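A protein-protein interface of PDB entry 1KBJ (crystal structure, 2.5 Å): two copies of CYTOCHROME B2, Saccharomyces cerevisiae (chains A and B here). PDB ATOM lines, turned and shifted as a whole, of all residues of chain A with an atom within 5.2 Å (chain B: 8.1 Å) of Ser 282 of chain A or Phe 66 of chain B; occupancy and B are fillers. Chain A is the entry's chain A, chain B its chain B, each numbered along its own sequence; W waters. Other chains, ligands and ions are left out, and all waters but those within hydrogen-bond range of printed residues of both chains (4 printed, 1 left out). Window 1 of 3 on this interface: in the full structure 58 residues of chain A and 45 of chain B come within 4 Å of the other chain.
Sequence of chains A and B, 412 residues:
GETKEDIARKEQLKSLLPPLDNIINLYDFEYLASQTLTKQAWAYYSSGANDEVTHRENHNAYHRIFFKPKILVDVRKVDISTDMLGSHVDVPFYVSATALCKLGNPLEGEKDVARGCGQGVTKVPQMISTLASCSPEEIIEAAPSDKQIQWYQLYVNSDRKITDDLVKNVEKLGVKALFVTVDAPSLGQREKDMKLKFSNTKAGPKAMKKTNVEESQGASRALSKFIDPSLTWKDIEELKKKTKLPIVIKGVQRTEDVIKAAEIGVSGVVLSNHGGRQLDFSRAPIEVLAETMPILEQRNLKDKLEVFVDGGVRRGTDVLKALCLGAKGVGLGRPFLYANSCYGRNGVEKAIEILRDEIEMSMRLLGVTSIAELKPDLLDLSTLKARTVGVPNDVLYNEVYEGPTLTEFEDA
O of Phe 281 of chain A is in hydrogen-bond range of N of Phe 67 of chain B (2.7 Å). The side-chain carboxylate (OD1) of Asp 380 of chain B is in salt-bridge range of the guanidinium group (NE) of Arg 283 of chain A (3.5 Å). OD1 of Asp 380 of chain B lies within salt-bridge range of NH2 of Arg 387 of chain A (3.3 Å). The side-chain hydroxyl of Thr 383 of chain B sits at hydrogen-bond distance from the guanidinium group of Arg 387 of chain A (2.9 Å).
The side-chain hydroxyl (OG1) of Thr 54 of chain A lies within hydrogen-bond range of the backbone carbonyl oxygen (O) of Ser 282 of chain A (2.7 Å). The side-chain amide oxygen (OE1) of Gln 253 of chain A lies within hydrogen-bond range of the side-chain hydroxyl (OG) of Ser 282 of chain A, at 2.7 Å. The backbone carbonyl oxygen (O) of Arg 283 of chain A lies close to the side-chain amide oxygen (OD1) of Asn 273 of chain A (3.2 Å).
Among the printed residues, pairs that only touch across the chains: Gln 253 of chain A with Pro 69 of chain B (3.4 Å), Leu 279 of chain A with Phe 67 of chain B (3.4 Å), Leu 279 of chain A with Pro 69 of chain B (3.9 Å), Leu 279 of chain A with Leu 365 of chain B (3.6 Å), Asp 280 of chain A with Phe 67 of chain B (3.4 Å), Phe 281 of chain A with His 63 of chain B (3.3 Å), Phe 281 of chain A with Ile 65 of chain B (3.5 Å), Phe 281 of chain A with Phe 66 of chain B (3.2 Å), Phe 281 of chain A with Lys 321 of chain B (3.3 Å), Ser 282 of chain A with Phe 66 of chain B (3.4 Å), Arg 283 of chain A with Phe 66 of chain B (3.8 Å), Arg 283 of chain A with Phe 67 of chain B (3.4 Å), Arg 283 of chain A with Lys 68 of chain B (3.4 Å) and Arg 387 of chain A with Phe 66 of chain B (3.6 Å).
Ser 282 of chain A touches just one residue of chain B: Phe 66 (3.4 Å). Printed residues of chain B within 4 Å of Arg 387 of chain A: Phe 66 (3.6 Å), Asp 380 (3.3 Å) and Thr 383 (2.9 Å). Of the printed residues of chain A, Asp 380 of chain B touches Arg 283 and Arg 387. Tyr 62 of chain B touches none of the printed residues of chain A. Leu 381 of chain B touches none of the printed residues of chain A. The nearest residue of chain B that does not touch Ser 282 of chain A is Phe 67 of chain B (4.2 Å). The nearest printed residue of chain B that does not touch Arg 283 of chain A is Pro 69 of chain B (5.8 Å).
Of the 12 printed residues of chain A, 7 touch a printed residue of chain B. Hydrophobic or aromatic side chains of chain A within 4 Å of the printed part of chain B: Leu 279 and Phe 281. Among the printed residues, 18 pairs touch across the chains. Among the printed residues, Asp or Glu carboxylates within 4 Å of a Lys or Arg side-chain nitrogen of the other chain: Arg 283 of chain A with Asp 380 of chain B (3.5 Å) and Arg 387 of chain A with Asp 380 of chain B (3.3 Å).
No position is printed for both chains.
Water W3 bridges OD1 of Asp 380 of chain B (2.7 Å) and NH2 of Arg 283 of chain A (2.9 Å). Water W2 lies within hydrogen-bond range of O of Arg 387 of chain A and O of Thr 383 of chain B. Water W4 lies within hydrogen-bond range of the backbone carbonyl oxygen (O) of Phe 67 of chain B (2.7 Å), the backbone carbonyl oxygen (O) of Gln 253 of chain A (2.8 Å), the backbone NH (N) of Arg 283 of chain A (3.0 Å) and the side-chain hydroxyl (OG) of Ser 282 of chain A (3.5 Å).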
ATOM      1  N   VAL A  53      -0.728 -21.707  12.454  1.00  0.00           N
ATOM      2  CA  VAL A  53      -1.618 -20.621  12.790  1.00  0.00           C
ATOM      3  C   VAL A  53      -2.890 -21.196  13.375  1.00  0.00           C
ATOM      4  O   VAL A  53      -3.310 -20.817  14.468  1.00  0.00           O
ATOM      5  CB  VAL A  53      -1.946 -19.773  11.537  1.00  0.00           C
ATOM      6  CG1 VAL A  53      -3.124 -18.849  11.809  1.00  0.00           C
ATOM      7  CG2 VAL A  53      -0.715 -18.998  11.108  1.00  0.00           C
ATOM      8  N   THR A  54      -3.507 -22.115  12.647  1.00  0.00           N
ATOM      9  CA  THR A  54      -4.733 -22.727  13.124  1.00  0.00           C
ATOM     10  C   THR A  54      -4.561 -23.409  14.491  1.00  0.00           C
ATOM     11  O   THR A  54      -5.434 -23.301  15.349  1.00  0.00           O
ATOM     12  CB  THR A  54      -5.267 -23.727  12.083  1.00  0.00           C
ATOM     13  OG1 THR A  54      -5.788 -22.996  10.978  1.00  0.00           O
ATOM     14  CG2 THR A  54      -6.381 -24.588  12.658  1.00  0.00           C
ATOM     15  N   GLU A  57      -4.760 -20.601  16.889  1.00  0.00           N
ATOM     16  CA  GLU A  57      -6.093 -19.998  16.787  1.00  0.00           C
ATOM     17  C   GLU A  57      -7.201 -20.869  17.446  1.00  0.00           C
ATOM     18  O   GLU A  57      -8.129 -20.337  18.052  1.00  0.00           O
ATOM     19  CB  GLU A  57      -6.420 -19.727  15.323  1.00  0.00           C
ATOM     20  CG  GLU A  57      -7.841 -19.291  15.036  1.00  0.00           C
ATOM     21  CD  GLU A  57      -8.209 -17.944  15.618  1.00  0.00           C
ATOM     22  OE1 GLU A  57      -7.307 -17.138  15.976  1.00  0.00           O
ATOM     23  OE2 GLU A  57      -9.427 -17.701  15.697  1.00  0.00           O
ATOM     24  N   GLN A 253     -15.219 -28.939   9.031  1.00  0.00           N
ATOM     25  CA  GLN A 253     -14.752 -27.575   9.201  1.00  0.00           C
ATOM     26  C   GLN A 253     -15.602 -26.460   8.596  1.00  0.00           C
ATOM     27  O   GLN A 253     -15.158 -25.330   8.506  1.00  0.00           O
ATOM     28  CB  GLN A 253     -13.326 -27.502   8.655  1.00  0.00           C
ATOM     29  CG  GLN A 253     -12.366 -28.435   9.394  1.00  0.00           C
ATOM     30  CD  GLN A 253     -11.216 -28.901   8.533  1.00  0.00           C
ATOM     31  OE1 GLN A 253     -10.250 -28.164   8.292  1.00  0.00           O
ATOM     32  NE2 GLN A 253     -11.321 -30.138   8.044  1.00  0.00           N
ATOM     33  N   ASN A 273     -10.066 -29.705  13.176  1.00  0.00           N
ATOM     34  CA  ASN A 273      -9.111 -29.526  12.105  1.00  0.00           C
ATOM     35  C   ASN A 273      -7.844 -30.288  12.434  1.00  0.00           C
ATOM     36  O   ASN A 273      -6.738 -29.919  12.012  1.00  0.00           O
ATOM     37  CB  ASN A 273      -8.815 -28.047  11.850  1.00  0.00           C
ATOM     38  CG  ASN A 273      -8.484 -27.290  13.109  1.00  0.00           C
ATOM     39  OD1 ASN A 273      -9.055 -26.239  13.369  1.00  0.00           O
ATOM     40  ND2 ASN A 273      -7.561 -27.805  13.889  1.00  0.00           N
ATOM     41  N   LEU A 279      -4.882 -28.598   7.459  1.00  0.00           N
ATOM     42  CA  LEU A 279      -4.966 -27.395   6.650  1.00  0.00           C
ATOM     43  C   LEU A 279      -4.685 -26.218   7.571  1.00  0.00           C
ATOM     44  O   LEU A 279      -5.353 -26.065   8.592  1.00  0.00           O
ATOM     45  CB  LEU A 279      -6.385 -27.228   6.082  1.00  0.00           C
ATOM     46  CG  LEU A 279      -6.614 -26.533   4.730  1.00  0.00           C
ATOM     47  CD1 LEU A 279      -7.862 -25.693   4.834  1.00  0.00           C
ATOM     48  CD2 LEU A 279      -5.433 -25.688   4.335  1.00  0.00           C
ATOM     49  N   ASP A 280      -3.692 -25.401   7.252  1.00  0.00           N
ATOM     50  CA  ASP A 280      -3.455 -24.246   8.085  1.00  0.00           C
ATOM     51  C   ASP A 280      -4.450 -23.179   7.591  1.00  0.00           C
ATOM     52  O   ASP A 280      -4.737 -23.072   6.400  1.00  0.00           O
ATOM     53  CB  ASP A 280      -2.003 -23.796   7.961  1.00  0.00           C
ATOM     54  CG  ASP A 280      -1.511 -23.060   9.204  1.00  0.00           C
ATOM     55  OD1 ASP A 280      -2.073 -23.267  10.298  1.00  0.00           O
ATOM     56  OD2 ASP A 280      -0.552 -22.281   9.080  1.00  0.00           O
ATOM     57  N   PHE A 281      -4.999 -22.426   8.523  1.00  0.00           N
ATOM     58  CA  PHE A 281      -5.994 -21.395   8.270  1.00  0.00           C
ATOM     59  C   PHE A 281      -7.402 -21.935   8.199  1.00  0.00           C
ATOM     60  O   PHE A 281      -8.317 -21.322   7.633  1.00  0.00           O
ATOM     61  CB  PHE A 281      -5.658 -20.525   7.063  1.00  0.00           C
ATOM     62  CG  PHE A 281      -4.689 -19.436   7.400  1.00  0.00           C
ATOM     63  CD1 PHE A 281      -5.106 -18.343   8.156  1.00  0.00           C
ATOM     64  CD2 PHE A 281      -3.326 -19.576   7.103  1.00  0.00           C
ATOM     65  CE1 PHE A 281      -4.172 -17.389   8.641  1.00  0.00           C
ATOM     66  CE2 PHE A 281      -2.394 -18.646   7.575  1.00  0.00           C
ATOM     67  CZ  PHE A 281      -2.820 -17.545   8.355  1.00  0.00           C
ATOM     68  N   SER A 282      -7.565 -23.104   8.795  1.00  0.00           N
ATOM     69  CA  SER A 282      -8.889 -23.661   8.939  1.00  0.00           C
ATOM     70  C   SER A 282      -9.323 -22.841  10.181  1.00  0.00           C
ATOM     71  O   SER A 282      -8.467 -22.380  10.924  1.00  0.00           O
ATOM     72  CB  SER A 282      -8.823 -25.149   9.277  1.00  0.00           C
ATOM     73  OG  SER A 282     -10.126 -25.696   9.282  1.00  0.00           O
ATOM     74  N   ARG A 283     -10.618 -22.627  10.398  1.00  0.00           N
ATOM     75  CA  ARG A 283     -11.049 -21.834  11.552  1.00  0.00           C
ATOM     76  C   ARG A 283     -11.079 -22.574  12.872  1.00  0.00           C
ATOM     77  O   ARG A 283     -11.064 -23.799  12.914  1.00  0.00           O
ATOM     78  CB  ARG A 283     -12.441 -21.268  11.341  1.00  0.00           C
ATOM     79  CG  ARG A 283     -12.546 -20.301  10.211  1.00  0.00           C
ATOM     80  CD  ARG A 283     -13.589 -20.795   9.297  1.00  0.00           C
ATOM     81  NE  ARG A 283     -14.917 -20.333   9.630  1.00  0.00           N
ATOM     82  CZ  ARG A 283     -16.010 -21.016   9.326  1.00  0.00           C
ATOM     83  NH1 ARG A 283     -15.922 -22.210   8.715  1.00  0.00           N
ATOM     84  NH2 ARG A 283     -17.193 -20.467   9.543  1.00  0.00           N
ATOM     85  N   ALA A 284     -11.111 -21.802  13.953  1.00  0.00           N
ATOM     86  CA  ALA A 284     -11.205 -22.382  15.281  1.00  0.00           C
ATOM     87  C   ALA A 284     -12.540 -23.132  15.307  1.00  0.00           C
ATOM     88  O   ALA A 284     -13.572 -22.588  14.913  1.00  0.00           O
ATOM     89  CB  ALA A 284     -11.208 -21.285  16.332  1.00  0.00           C
ATOM     90  N   ARG A 387     -11.449 -11.256  15.337  1.00  0.00           N
ATOM     91  CA  ARG A 387     -10.242 -12.015  15.015  1.00  0.00           C
ATOM     92  C   ARG A 387      -9.463 -10.999  14.152  1.00  0.00           C
ATOM     93  O   ARG A 387      -9.773 -10.764  12.974  1.00  0.00           O
ATOM     94  CB  ARG A 387     -10.624 -13.260  14.207  1.00  0.00           C
ATOM     95  CG  ARG A 387      -9.449 -14.005  13.597  1.00  0.00           C
ATOM     96  CD  ARG A 387      -9.818 -14.476  12.200  1.00  0.00           C
ATOM     97  NE  ARG A 387     -10.662 -15.655  12.251  1.00  0.00           N
ATOM     98  CZ  ARG A 387     -11.553 -16.003  11.328  1.00  0.00           C
ATOM     99  NH1 ARG A 387     -11.754 -15.272  10.248  1.00  0.00           N
ATOM    100  NH2 ARG A 387     -12.255 -17.103  11.502  1.00  0.00           N
ATOM    101  N   ALA B  61      -2.081  -9.307   5.426  1.00  0.00           N
ATOM    102  CA  ALA B  61      -3.496  -9.280   5.039  1.00  0.00           C
ATOM    103  C   ALA B  61      -3.983 -10.669   4.634  1.00  0.00           C
ATOM    104  O   ALA B  61      -5.173 -10.999   4.735  1.00  0.00           O
ATOM    105  CB  ALA B  61      -3.723  -8.302   3.919  1.00  0.00           C
ATOM    106  N   TYR B  62      -3.070 -11.507   4.179  1.00  0.00           N
ATOM    107  CA  TYR B  62      -3.507 -12.845   3.837  1.00  0.00           C
ATOM    108  C   TYR B  62      -4.043 -13.559   5.090  1.00  0.00           C
ATOM    109  O   TYR B  62      -4.869 -14.475   4.993  1.00  0.00           O
ATOM    110  CB  TYR B  62      -2.349 -13.622   3.234  1.00  0.00           C
ATOM    111  CG  TYR B  62      -2.132 -13.334   1.750  1.00  0.00           C
ATOM    112  CD1 TYR B  62      -2.905 -13.978   0.770  1.00  0.00           C
ATOM    113  CD2 TYR B  62      -1.193 -12.378   1.329  1.00  0.00           C
ATOM    114  CE1 TYR B  62      -2.753 -13.675  -0.578  1.00  0.00           C
ATOM    115  CE2 TYR B  62      -1.044 -12.067  -0.019  1.00  0.00           C
ATOM    116  CZ  TYR B  62      -1.826 -12.716  -0.958  1.00  0.00           C
ATOM    117  OH  TYR B  62      -1.690 -12.388  -2.274  1.00  0.00           O
ATOM    118  N   HIS B  63      -3.607 -13.116   6.267  1.00  0.00           N
ATOM    119  CA  HIS B  63      -4.029 -13.780   7.483  1.00  0.00           C
ATOM    120  C   HIS B  63      -5.364 -13.327   8.031  1.00  0.00           C
ATOM    121  O   HIS B  63      -5.835 -13.830   9.057  1.00  0.00           O
ATOM    122  CB  HIS B  63      -2.939 -13.697   8.537  1.00  0.00           C
ATOM    123  CG  HIS B  63      -1.696 -14.419   8.140  1.00  0.00           C
ATOM    124  ND1 HIS B  63      -0.667 -14.672   9.020  1.00  0.00           N
ATOM    125  CD2 HIS B  63      -1.325 -14.967   6.955  1.00  0.00           C
ATOM    126  CE1 HIS B  63       0.284 -15.347   8.395  1.00  0.00           C
ATOM    127  NE2 HIS B  63      -0.091 -15.539   7.140  1.00  0.00           N
ATOM    128  N   ARG B  64      -5.986 -12.404   7.318  1.00  0.00           N
ATOM    129  CA  ARG B  64      -7.304 -11.933   7.700  1.00  0.00           C
ATOM    130  C   ARG B  64      -8.312 -12.810   6.947  1.00  0.00           C
ATOM    131  O   ARG B  64      -9.525 -12.593   7.003  1.00  0.00           O
ATOM    132  CB  ARG B  64      -7.503 -10.455   7.311  1.00  0.00           C
ATOM    133  CG  ARG B  64      -6.657  -9.486   8.099  1.00  0.00           C
ATOM    134  CD  ARG B  64      -7.087  -7.994   7.953  1.00  0.00           C
ATOM    135  NE  ARG B  64      -6.088  -7.186   8.642  1.00  0.00           N
ATOM    136  CZ  ARG B  64      -5.055  -6.610   8.041  1.00  0.00           C
ATOM    137  NH1 ARG B  64      -4.918  -6.729   6.725  1.00  0.00           N
ATOM    138  NH2 ARG B  64      -4.117  -5.995   8.765  1.00  0.00           N
ATOM    139  N   ILE B  65      -7.803 -13.802   6.226  1.00  0.00           N
ATOM    140  CA  ILE B  65      -8.677 -14.696   5.480  1.00  0.00           C
ATOM    141  C   ILE B  65      -8.484 -16.119   5.947  1.00  0.00           C
ATOM    142  O   ILE B  65      -7.356 -16.582   6.069  1.00  0.00           O
ATOM    143  CB  ILE B  65      -8.364 -14.670   3.977  1.00  0.00           C
ATOM    144  CG1 ILE B  65      -8.616 -13.282   3.427  1.00  0.00           C
ATOM    145  CG2 ILE B  65      -9.185 -15.736   3.252  1.00  0.00           C
ATOM    146  CD1 ILE B  65      -7.989 -13.063   2.065  1.00  0.00           C
ATOM    147  N   PHE B  66      -9.592 -16.808   6.188  1.00  0.00           N
ATOM    148  CA  PHE B  66      -9.559 -18.188   6.622  1.00  0.00           C
ATOM    149  C   PHE B  66     -10.279 -19.095   5.622  1.00  0.00           C
ATOM    150  O   PHE B  66     -10.985 -18.621   4.735  1.00  0.00           O
ATOM    151  CB  PHE B  66     -10.150 -18.310   8.036  1.00  0.00           C
ATOM    152  CG  PHE B  66      -9.133 -18.083   9.138  1.00  0.00           C
ATOM    153  CD1 PHE B  66      -8.593 -16.807   9.371  1.00  0.00           C
ATOM    154  CD2 PHE B  66      -8.684 -19.146   9.929  1.00  0.00           C
ATOM    155  CE1 PHE B  66      -7.614 -16.591  10.371  1.00  0.00           C
ATOM    156  CE2 PHE B  66      -7.699 -18.932  10.937  1.00  0.00           C
ATOM    157  CZ  PHE B  66      -7.168 -17.647  11.150  1.00  0.00           C
ATOM    158  N   PHE B  67     -10.075 -20.402   5.757  1.00  0.00           N
ATOM    159  CA  PHE B  67     -10.670 -21.389   4.860  1.00  0.00           C
ATOM    160  C   PHE B  67     -11.906 -22.070   5.402  1.00  0.00           C
ATOM    161  O   PHE B  67     -12.053 -22.251   6.602  1.00  0.00           O
ATOM    162  CB  PHE B  67      -9.682 -22.509   4.555  1.00  0.00           C
ATOM    163  CG  PHE B  67      -8.505 -22.088   3.758  1.00  0.00           C
ATOM    164  CD1 PHE B  67      -7.203 -22.389   4.205  1.00  0.00           C
ATOM    165  CD2 PHE B  67      -8.673 -21.398   2.547  1.00  0.00           C
ATOM    166  CE1 PHE B  67      -6.092 -21.994   3.453  1.00  0.00           C
ATOM    167  CE2 PHE B  67      -7.558 -21.002   1.783  1.00  0.00           C
ATOM    168  CZ  PHE B  67      -6.270 -21.296   2.233  1.00  0.00           C
ATOM    169  N   LYS B  68     -12.761 -22.482   4.474  1.00  0.00           N
ATOM    170  CA  LYS B  68     -13.982 -23.213   4.765  1.00  0.00           C
ATOM    171  C   LYS B  68     -13.870 -24.421   3.832  1.00  0.00           C
ATOM    172  O   LYS B  68     -14.589 -24.535   2.836  1.00  0.00           O
ATOM    173  CB  LYS B  68     -15.193 -22.342   4.437  1.00  0.00           C
ATOM    174  CG  LYS B  68     -15.446 -21.297   5.510  1.00  0.00           C
ATOM    175  CD  LYS B  68     -16.423 -20.226   5.092  1.00  0.00           C
ATOM    176  CE  LYS B  68     -17.650 -20.746   4.386  1.00  0.00           C
ATOM    177  NZ  LYS B  68     -18.648 -19.648   4.223  1.00  0.00           N
ATOM    178  N   PRO B  69     -12.957 -25.350   4.158  1.00  0.00           N
ATOM    179  CA  PRO B  69     -12.671 -26.573   3.399  1.00  0.00           C
ATOM    180  C   PRO B  69     -13.788 -27.593   3.329  1.00  0.00           C
ATOM    181  O   PRO B  69     -14.551 -27.758   4.289  1.00  0.00           O
ATOM    182  CB  PRO B  69     -11.460 -27.129   4.121  1.00  0.00           C
ATOM    183  CG  PRO B  69     -11.791 -26.837   5.535  1.00  0.00           C
ATOM    184  CD  PRO B  69     -12.298 -25.407   5.476  1.00  0.00           C
ATOM    185  N   THR B 317      -0.856 -21.544   0.711  1.00  0.00           N
ATOM    186  CA  THR B 317      -2.191 -21.100   1.095  1.00  0.00           C
ATOM    187  C   THR B 317      -2.400 -19.620   0.750  1.00  0.00           C
ATOM    188  O   THR B 317      -3.543 -19.203   0.510  1.00  0.00           O
ATOM    189  CB  THR B 317      -2.485 -21.353   2.592  1.00  0.00           C
ATOM    190  OG1 THR B 317      -1.449 -20.781   3.378  1.00  0.00           O
ATOM    191  CG2 THR B 317      -2.553 -22.851   2.897  1.00  0.00           C
ATOM    192  N   LYS B 321      -5.646 -18.523  -1.527  1.00  0.00           N
ATOM    193  CA  LYS B 321      -6.585 -17.470  -1.204  1.00  0.00           C
ATOM    194  C   LYS B 321      -6.694 -16.515  -2.403  1.00  0.00           C
ATOM    195  O   LYS B 321      -7.789 -16.229  -2.858  1.00  0.00           O
ATOM    196  CB  LYS B 321      -6.152 -16.731   0.068  1.00  0.00           C
ATOM    197  CG  LYS B 321      -6.076 -17.638   1.271  1.00  0.00           C
ATOM    198  CD  LYS B 321      -5.359 -16.984   2.448  1.00  0.00           C
ATOM    199  CE  LYS B 321      -5.637 -17.740   3.734  1.00  0.00           C
ATOM    200  NZ  LYS B 321      -4.834 -17.234   4.886  1.00  0.00           N
ATOM    201  N   CYS B 324      -8.796 -18.146  -5.032  1.00  0.00           N
ATOM    202  CA  CYS B 324     -10.216 -18.230  -4.686  1.00  0.00           C
ATOM    203  C   CYS B 324     -10.913 -16.887  -4.867  1.00  0.00           C
ATOM    204  O   CYS B 324     -12.110 -16.847  -5.159  1.00  0.00           O
ATOM    205  CB  CYS B 324     -10.413 -18.694  -3.247  1.00  0.00           C
ATOM    206  SG  CYS B 324     -10.029 -20.432  -2.962  1.00  0.00           S
ATOM    207  N   LEU B 365      -6.614 -30.675   1.002  1.00  0.00           N
ATOM    208  CA  LEU B 365      -7.266 -30.475   2.294  1.00  0.00           C
ATOM    209  C   LEU B 365      -8.397 -29.457   2.181  1.00  0.00           C
ATOM    210  O   LEU B 365      -9.299 -29.430   3.026  1.00  0.00           O
ATOM    211  CB  LEU B 365      -6.227 -30.054   3.354  1.00  0.00           C
ATOM    212  CG  LEU B 365      -5.094 -31.093   3.569  1.00  0.00           C
ATOM    213  CD1 LEU B 365      -4.111 -30.671   4.672  1.00  0.00           C
ATOM    214  CD2 LEU B 365      -5.726 -32.417   3.923  1.00  0.00           C
ATOM    215  N   LEU B 366      -8.348 -28.634   1.130  1.00  0.00           N
ATOM    216  CA  LEU B 366      -9.385 -27.645   0.862  1.00  0.00           C
ATOM    217  C   LEU B 366     -10.573 -28.375   0.270  1.00  0.00           C
ATOM    218  O   LEU B 366     -11.707 -27.894   0.323  1.00  0.00           O
ATOM    219  CB  LEU B 366      -8.909 -26.612  -0.151  1.00  0.00           C
ATOM    220  CG  LEU B 366      -8.790 -25.178   0.323  1.00  0.00           C
ATOM    221  CD1 LEU B 366      -8.602 -24.296  -0.897  1.00  0.00           C
ATOM    222  CD2 LEU B 366     -10.040 -24.763   1.107  1.00  0.00           C
ATOM    223  N   PRO B 376     -14.716 -18.221  -4.210  1.00  0.00           N
ATOM    224  CA  PRO B 376     -14.811 -17.626  -2.884  1.00  0.00           C
ATOM    225  C   PRO B 376     -15.616 -18.357  -1.830  1.00  0.00           C
ATOM    226  O   PRO B 376     -15.444 -18.089  -0.644  1.00  0.00           O
ATOM    227  CB  PRO B 376     -15.286 -16.194  -3.172  1.00  0.00           C
ATOM    228  CG  PRO B 376     -15.963 -16.301  -4.494  1.00  0.00           C
ATOM    229  CD  PRO B 376     -15.162 -17.287  -5.258  1.00  0.00           C
ATOM    230  N   ASP B 377     -16.509 -19.265  -2.200  1.00  0.00           N
ATOM    231  CA  ASP B 377     -17.258 -19.930  -1.130  1.00  0.00           C
ATOM    232  C   ASP B 377     -16.312 -20.782  -0.279  1.00  0.00           C
ATOM    233  O   ASP B 377     -16.677 -21.248   0.799  1.00  0.00           O
ATOM    234  CB  ASP B 377     -18.423 -20.771  -1.675  1.00  0.00           C
ATOM    235  CG  ASP B 377     -19.467 -21.112  -0.587  1.00  0.00           C
ATOM    236  OD1 ASP B 377     -19.931 -20.185   0.119  1.00  0.00           O
ATOM    237  OD2 ASP B 377     -19.835 -22.311  -0.445  1.00  0.00           O
ATOM    238  N   LEU B 378     -15.087 -20.973  -0.754  1.00  0.00           N
ATOM    239  CA  LEU B 378     -14.116 -21.736   0.021  1.00  0.00           C
ATOM    240  C   LEU B 378     -13.439 -20.882   1.081  1.00  0.00           C
ATOM    241  O   LEU B 378     -12.743 -21.399   1.955  1.00  0.00           O
ATOM    242  CB  LEU B 378     -13.043 -22.308  -0.898  1.00  0.00           C
ATOM    243  CG  LEU B 378     -13.469 -23.401  -1.878  1.00  0.00           C
ATOM    244  CD1 LEU B 378     -12.328 -23.646  -2.840  1.00  0.00           C
ATOM    245  CD2 LEU B 378     -13.820 -24.677  -1.109  1.00  0.00           C
ATOM    246  N   LEU B 379     -13.621 -19.573   0.998  1.00  0.00           N
ATOM    247  CA  LEU B 379     -12.983 -18.695   1.952  1.00  0.00           C
ATOM    248  C   LEU B 379     -13.946 -18.107   2.963  1.00  0.00           C
ATOM    249  O   LEU B 379     -15.138 -17.942   2.670  1.00  0.00           O
ATOM    250  CB  LEU B 379     -12.305 -17.524   1.229  1.00  0.00           C
ATOM    251  CG  LEU B 379     -11.338 -17.795   0.085  1.00  0.00           C
ATOM    252  CD1 LEU B 379     -10.842 -16.466  -0.506  1.00  0.00           C
ATOM    253  CD2 LEU B 379     -10.195 -18.626   0.589  1.00  0.00           C
ATOM    254  N   ASP B 380     -13.425 -17.811   4.154  1.00  0.00           N
ATOM    255  CA  ASP B 380     -14.213 -17.121   5.175  1.00  0.00           C
ATOM    256  C   ASP B 380     -13.679 -15.694   5.045  1.00  0.00           C
ATOM    257  O   ASP B 380     -12.536 -15.434   5.407  1.00  0.00           O
ATOM    258  CB  ASP B 380     -13.916 -17.616   6.581  1.00  0.00           C
ATOM    259  CG  ASP B 380     -14.554 -16.743   7.645  1.00  0.00           C
ATOM    260  OD1 ASP B 380     -14.257 -16.975   8.825  1.00  0.00           O
ATOM    261  OD2 ASP B 380     -15.353 -15.824   7.321  1.00  0.00           O
ATOM    262  N   LEU B 381     -14.493 -14.777   4.519  1.00  0.00           N
ATOM    263  CA  LEU B 381     -14.033 -13.408   4.318  1.00  0.00           C
ATOM    264  C   LEU B 381     -14.604 -12.453   5.353  1.00  0.00           C
ATOM    265  O   LEU B 381     -14.386 -11.257   5.269  1.00  0.00           O
ATOM    266  CB  LEU B 381     -14.434 -12.925   2.922  1.00  0.00           C
ATOM    267  CG  LEU B 381     -13.861 -13.729   1.748  1.00  0.00           C
ATOM    268  CD1 LEU B 381     -14.517 -13.293   0.433  1.00  0.00           C
ATOM    269  CD2 LEU B 381     -12.365 -13.550   1.670  1.00  0.00           C
ATOM    270  N   SER B 382     -15.325 -12.983   6.328  1.00  0.00           N
ATOM    271  CA  SER B 382     -15.959 -12.147   7.342  1.00  0.00           C
ATOM    272  C   SER B 382     -15.046 -11.217   8.137  1.00  0.00           C
ATOM    273  O   SER B 382     -15.512 -10.236   8.709  1.00  0.00           O
ATOM    274  CB  SER B 382     -16.728 -13.021   8.329  1.00  0.00           C
ATOM    275  OG  SER B 382     -15.824 -13.859   9.018  1.00  0.00           O
ATOM    276  N   THR B 383     -13.758 -11.502   8.201  1.00  0.00           N
ATOM    277  CA  THR B 383     -12.895 -10.618   8.975  1.00  0.00           C
ATOM    278  C   THR B 383     -11.800 -10.011   8.110  1.00  0.00           C
ATOM    279  O   THR B 383     -10.754  -9.598   8.591  1.00  0.00           O
ATOM    280  CB  THR B 383     -12.273 -11.367  10.183  1.00  0.00           C
ATOM    281  OG1 THR B 383     -11.423 -12.415   9.708  1.00  0.00           O
ATOM    282  CG2 THR B 383     -13.380 -11.975  11.069  1.00  0.00           C
ATOM    283  N   LEU B 384     -12.059  -9.948   6.815  1.00  0.00           N
ATOM    284  CA  LEU B 384     -11.089  -9.383   5.902  1.00  0.00           C
ATOM    285  C   LEU B 384     -10.746  -7.945   6.282  1.00  0.00           C
ATOM    286  O   LEU B 384      -9.628  -7.484   6.077  1.00  0.00           O
ATOM    287  CB  LEU B 384     -11.640  -9.411   4.479  1.00  0.00           C
ATOM    288  CG  LEU B 384     -10.642  -8.883   3.455  1.00  0.00           C
ATOM    289  CD1 LEU B 384      -9.392  -9.693   3.514  1.00  0.00           C
ATOM    290  CD2 LEU B 384     -11.231  -8.965   2.085  1.00  0.00           C
HETATM  291  O   HOH W   1     -15.636 -29.372   6.223  1.00  0.00           O
HETATM  292  O   HOH W   2      -8.857 -10.571  10.445  1.00  0.00           O
HETATM  293  O   HOH W   3     -16.360 -17.800  10.229  1.00  0.00           O
HETATM  294  O   HOH W   4     -12.898 -23.702   8.777  1.00  0.00           O
